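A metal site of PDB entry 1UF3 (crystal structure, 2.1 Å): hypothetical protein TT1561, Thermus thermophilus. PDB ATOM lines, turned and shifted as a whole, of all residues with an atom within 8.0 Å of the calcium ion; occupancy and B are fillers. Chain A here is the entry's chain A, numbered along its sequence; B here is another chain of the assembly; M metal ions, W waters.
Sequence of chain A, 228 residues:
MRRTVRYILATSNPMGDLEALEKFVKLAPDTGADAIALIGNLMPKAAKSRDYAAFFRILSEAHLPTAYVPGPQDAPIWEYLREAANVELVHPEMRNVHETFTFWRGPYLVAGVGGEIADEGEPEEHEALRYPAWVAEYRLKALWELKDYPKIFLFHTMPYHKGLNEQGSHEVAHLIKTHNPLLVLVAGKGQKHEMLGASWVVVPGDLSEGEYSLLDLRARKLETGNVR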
ATOM      1  N   ARG A   3       8.848   9.621 -11.651  1.00  0.00           N
ATOM      2  CA  ARG A   3      10.017  10.342 -11.159  1.00  0.00           C
ATOM      3  C   ARG A   3       9.737  11.838 -11.054  1.00  0.00           C
ATOM      4  O   ARG A   3       8.607  12.268 -11.336  1.00  0.00           O
ATOM      5  CB  ARG A   3      11.195  10.069 -12.075  1.00  0.00           C
ATOM      6  CG  ARG A   3      11.585   8.577 -12.063  1.00  0.00           C
ATOM      7  CD  ARG A   3      12.688   8.268 -13.044  1.00  0.00           C
ATOM      8  NE  ARG A   3      12.893   6.823 -13.177  1.00  0.00           N
ATOM      9  CZ  ARG A   3      13.328   6.034 -12.209  1.00  0.00           C
ATOM     10  NH1 ARG A   3      13.615   6.540 -11.008  1.00  0.00           N
ATOM     11  NH2 ARG A   3      13.499   4.734 -12.432  1.00  0.00           N
ATOM     12  N   THR A   4      10.721  12.628 -10.639  1.00  0.00           N
ATOM     13  CA  THR A   4      10.522  14.074 -10.470  1.00  0.00           C
ATOM     14  C   THR A   4      10.194  14.748 -11.793  1.00  0.00           C
ATOM     15  O   THR A   4      10.596  14.301 -12.850  1.00  0.00           O
ATOM     16  CB  THR A   4      11.771  14.784  -9.930  1.00  0.00           C
ATOM     17  OG1 THR A   4      12.942  14.147 -10.483  1.00  0.00           O
ATOM     18  CG2 THR A   4      11.797  14.760  -8.420  1.00  0.00           C
ATOM     19  N   VAL A   5       9.439  15.830 -11.729  1.00  0.00           N
ATOM     20  CA  VAL A   5       9.099  16.538 -12.943  1.00  0.00           C
ATOM     21  C   VAL A   5      10.204  17.518 -13.339  1.00  0.00           C
ATOM     22  O   VAL A   5      10.553  18.400 -12.556  1.00  0.00           O
ATOM     23  CB  VAL A   5       7.832  17.360 -12.738  1.00  0.00           C
ATOM     24  CG1 VAL A   5       7.594  18.250 -13.989  1.00  0.00           C
ATOM     25  CG2 VAL A   5       6.657  16.438 -12.476  1.00  0.00           C
ATOM     26  N   ARG A   6      10.759  17.362 -14.537  1.00  0.00           N
ATOM     27  CA  ARG A   6      11.780  18.261 -15.047  1.00  0.00           C
ATOM     28  C   ARG A   6      11.296  18.929 -16.336  1.00  0.00           C
ATOM     29  O   ARG A   6      11.505  20.124 -16.534  1.00  0.00           O
ATOM     30  CB  ARG A   6      13.111  17.544 -15.325  1.00  0.00           C
ATOM     31  CG  ARG A   6      14.164  18.522 -15.915  1.00  0.00           C
ATOM     32  CD  ARG A   6      15.622  17.974 -15.935  1.00  0.00           C
ATOM     33  NE  ARG A   6      16.473  18.874 -16.707  1.00  0.00           N
ATOM     34  CZ  ARG A   6      17.667  18.559 -17.215  1.00  0.00           C
ATOM     35  NH1 ARG A   6      18.186  17.360 -17.032  1.00  0.00           N
ATOM     36  NH2 ARG A   6      18.317  19.449 -17.969  1.00  0.00           N
ATOM     37  N   TYR A   7      10.663  18.130 -17.203  1.00  0.00           N
ATOM     38  CA  TYR A   7      10.156  18.618 -18.478  1.00  0.00           C
ATOM     39  C   TYR A   7       8.644  18.650 -18.506  1.00  0.00           C
ATOM     40  O   TYR A   7       7.980  17.676 -18.130  1.00  0.00           O
ATOM     41  CB  TYR A   7      10.680  17.757 -19.624  1.00  0.00           C
ATOM     42  CG  TYR A   7      12.170  17.783 -19.695  1.00  0.00           C
ATOM     43  CD1 TYR A   7      12.944  16.847 -18.986  1.00  0.00           C
ATOM     44  CD2 TYR A   7      12.828  18.798 -20.390  1.00  0.00           C
ATOM     45  CE1 TYR A   7      14.324  16.936 -18.972  1.00  0.00           C
ATOM     46  CE2 TYR A   7      14.211  18.907 -20.367  1.00  0.00           C
ATOM     47  CZ  TYR A   7      14.961  17.973 -19.655  1.00  0.00           C
ATOM     48  OH  TYR A   7      16.314  18.106 -19.598  1.00  0.00           O
ATOM     49  N   ALA A  28       3.984  13.436 -26.096  1.00  0.00           N
ATOM     50  CA  ALA A  28       4.560  13.196 -24.784  1.00  0.00           C
ATOM     51  C   ALA A  28       5.558  12.040 -24.690  1.00  0.00           C
ATOM     52  O   ALA A  28       6.644  12.223 -24.172  1.00  0.00           O
ATOM     53  CB  ALA A  28       3.442  13.037 -23.738  1.00  0.00           C
ATOM     54  N   PRO A  29       5.211  10.840 -25.196  1.00  0.00           N
ATOM     55  CA  PRO A  29       6.193   9.757 -25.061  1.00  0.00           C
ATOM     56  C   PRO A  29       7.448  10.033 -25.859  1.00  0.00           C
ATOM     57  O   PRO A  29       8.547   9.704 -25.441  1.00  0.00           O
ATOM     58  CB  PRO A  29       5.452   8.516 -25.572  1.00  0.00           C
ATOM     59  CG  PRO A  29       3.988   8.846 -25.332  1.00  0.00           C
ATOM     60  CD  PRO A  29       3.927  10.329 -25.727  1.00  0.00           C
ATOM     61  N   THR A  31       8.822  12.914 -26.536  1.00  0.00           N
ATOM     62  CA  THR A  31       9.668  13.939 -25.917  1.00  0.00           C
ATOM     63  C   THR A  31      10.201  13.557 -24.540  1.00  0.00           C
ATOM     64  O   THR A  31      11.225  14.068 -24.105  1.00  0.00           O
ATOM     65  CB  THR A  31       8.944  15.282 -25.757  1.00  0.00           C
ATOM     66  OG1 THR A  31       7.836  15.134 -24.859  1.00  0.00           O
ATOM     67  CG2 THR A  31       8.445  15.776 -27.088  1.00  0.00           C
ATOM     68  N   GLY A  32       9.534  12.645 -23.857  1.00  0.00           N
ATOM     69  CA  GLY A  32       9.987  12.251 -22.529  1.00  0.00           C
ATOM     70  C   GLY A  32       9.381  13.157 -21.477  1.00  0.00           C
ATOM     71  O   GLY A  32       9.772  13.094 -20.311  1.00  0.00           O
ATOM     72  N   ALA A  33       8.440  14.003 -21.875  1.00  0.00           N
ATOM     73  CA  ALA A  33       7.780  14.916 -20.930  1.00  0.00           C
ATOM     74  C   ALA A  33       7.391  14.192 -19.647  1.00  0.00           C
ATOM     75  O   ALA A  33       6.996  13.015 -19.691  1.00  0.00           O
ATOM     76  CB  ALA A  33       6.537  15.493 -21.559  1.00  0.00           C
ATOM     77  N   ASP A  34       7.485  14.902 -18.518  1.00  0.00           N
ATOM     78  CA  ASP A  34       7.143  14.335 -17.212  1.00  0.00           C
ATOM     79  C   ASP A  34       5.778  14.768 -16.774  1.00  0.00           C
ATOM     80  O   ASP A  34       5.152  14.129 -15.912  1.00  0.00           O
ATOM     81  CB  ASP A  34       8.160  14.769 -16.175  1.00  0.00           C
ATOM     82  CG  ASP A  34       9.558  14.469 -16.609  1.00  0.00           C
ATOM     83  OD1 ASP A  34       9.801  13.301 -17.002  1.00  0.00           O
ATOM     84  OD2 ASP A  34      10.382  15.402 -16.606  1.00  0.00           O
ATOM     85  N   ALA A  35       5.306  15.865 -17.371  1.00  0.00           N
ATOM     86  CA  ALA A  35       3.998  16.371 -17.061  1.00  0.00           C
ATOM     87  C   ALA A  35       3.431  17.188 -18.246  1.00  0.00           C
ATOM     88  O   ALA A  35       4.150  17.469 -19.210  1.00  0.00           O
ATOM     89  CB  ALA A  35       4.065  17.210 -15.836  1.00  0.00           C
ATOM     90  N   LEU A  64       0.011  10.831 -17.635  1.00  0.00           N
ATOM     91  CA  LEU A  64       1.053  11.682 -17.047  1.00  0.00           C
ATOM     92  C   LEU A  64       0.425  12.756 -16.175  1.00  0.00           C
ATOM     93  O   LEU A  64      -0.712  13.168 -16.410  1.00  0.00           O
ATOM     94  CB  LEU A  64       1.868  12.429 -18.143  1.00  0.00           C
ATOM     95  CG  LEU A  64       2.885  11.763 -19.095  1.00  0.00           C
ATOM     96  CD1 LEU A  64       3.310  12.788 -20.140  1.00  0.00           C
ATOM     97  CD2 LEU A  64       4.109  11.228 -18.321  1.00  0.00           C
ATOM     98  N   MET B   1      12.881  13.189 -17.482  1.00  0.00           N
ATOM     99  CA  MET B   1      14.088  13.352 -18.342  1.00  0.00           C
ATOM    100  C   MET B   1      13.711  13.144 -19.813  1.00  0.00           C
ATOM    101  O   MET B   1      12.747  12.428 -20.117  1.00  0.00           O
ATOM    102  CB  MET B   1      15.172  12.347 -17.946  1.00  0.00           C
ATOM    103  CG  MET B   1      15.752  12.511 -16.528  1.00  0.00           C
ATOM    104  SD  MET B   1      16.619  14.251 -16.162  1.00  0.00           S
ATOM    105  CE  MET B   1      18.322  13.905 -17.080  1.00  0.00           C
ATOM    106  N   ARG B   2      14.460  13.774 -20.708  1.00  0.00           N
ATOM    107  CA  ARG B   2      14.202  13.602 -22.129  1.00  0.00           C
ATOM    108  C   ARG B   2      14.308  12.109 -22.439  1.00  0.00           C
ATOM    109  O   ARG B   2      14.963  11.342 -21.724  1.00  0.00           O
ATOM    110  CB  ARG B   2      15.232  14.379 -22.959  1.00  0.00           C
ATOM    111  CG  ARG B   2      15.111  15.912 -22.870  1.00  0.00           C
ATOM    112  CD  ARG B   2      16.213  16.602 -23.720  1.00  0.00           C
ATOM    113  NE  ARG B   2      15.985  18.032 -23.930  1.00  0.00           N
ATOM    114  CZ  ARG B   2      16.634  19.010 -23.302  1.00  0.00           C
ATOM    115  NH1 ARG B   2      17.584  18.749 -22.397  1.00  0.00           N
ATOM    116  NH2 ARG B   2      16.332  20.273 -23.576  1.00  0.00           N
ATOM    117  N   ARG B   3      13.667  11.692 -23.526  1.00  0.00           N
ATOM    118  CA  ARG B   3      13.674  10.299 -23.913  1.00  0.00           C
ATOM    119  C   ARG B   3      15.056   9.846 -24.307  1.00  0.00           C
ATOM    120  O   ARG B   3      15.474   8.731 -23.993  1.00  0.00           O
ATOM    121  CB  ARG B   3      12.710  10.062 -25.094  1.00  0.00           C
ATOM    122  CG  ARG B   3      12.729   8.617 -25.614  1.00  0.00           C
ATOM    123  CD  ARG B   3      11.649   8.358 -26.678  1.00  0.00           C
ATOM    124  NE  ARG B   3      11.906   9.093 -27.908  1.00  0.00           N
ATOM    125  CZ  ARG B   3      12.661   8.631 -28.899  1.00  0.00           C
ATOM    126  NH1 ARG B   3      13.225   7.436 -28.823  1.00  0.00           N
ATOM    127  NH2 ARG B   3      12.874   9.397 -29.960  1.00  0.00           N
ATOM    128  N   ARG B 105      19.777   7.216 -21.123  1.00  0.00           N
ATOM    129  CA  ARG B 105      18.514   7.350 -21.858  1.00  0.00           C
ATOM    130  C   ARG B 105      18.802   7.381 -23.357  1.00  0.00           C
ATOM    131  O   ARG B 105      19.657   8.139 -23.841  1.00  0.00           O
ATOM    132  CB  ARG B 105      17.812   8.642 -21.448  1.00  0.00           C
ATOM    133  CG  ARG B 105      17.446   8.718 -20.008  1.00  0.00           C
ATOM    134  CD  ARG B 105      16.055   8.207 -19.771  1.00  0.00           C
ATOM    135  NE  ARG B 105      15.266   9.171 -18.992  1.00  0.00           N
ATOM    136  CZ  ARG B 105      13.962   9.404 -19.184  1.00  0.00           C
ATOM    137  NH1 ARG B 105      13.300   8.760 -20.139  1.00  0.00           N
ATOM    138  NH2 ARG B 105      13.330  10.285 -18.411  1.00  0.00           N
HETATM  139 CA    CA M   1      10.788  11.956 -18.409  1.00  0.00          CA
HETATM  140  O   HOH W   1      10.949   9.893 -19.567  1.00  0.00           O
HETATM  141  O   HOH W   2       8.476  10.850 -18.565  1.00  0.00           O
HETATM  142  O   HOH W   3      11.444  10.526 -16.497  1.00  0.00           O
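O of Met 1 of chain B sits close to NH2 of Arg 105 of chain B (2.8 Å).
The backbone NH (N) of Tyr 7 sits at hydrogen-bond distance from the side-chain carboxylate (OD2) of Asp 34, at 2.8 Å.
NH1 of Arg 6 sits close to SD of Met 1 of chain B, at 3.6 Å.
NH1 of Arg 105 of chain B sits close to O of Arg 2 of chain B, 3.5 Å away.
The side-chain carboxylate of Asp 34 is in hydrogen-bond range of the backbone NH of Arg 6 (2.9 Å).
The calcium ion is bound by OD1 of Asp 34 (2.2 Å), water W1 (2.4 Å), O of Gly 32 (2.4 Å), water W3 (2.5 Å), water W2 (2.6 Å), N of Met 1 of chain B (2.6 Å) and O of Met 1 of chain B (2.6 Å).
The calcium ion has seven donor atoms within binding distance.
Slightly farther from the calcium ion lies NH2 of Arg 105 of chain B (3.0 Å).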
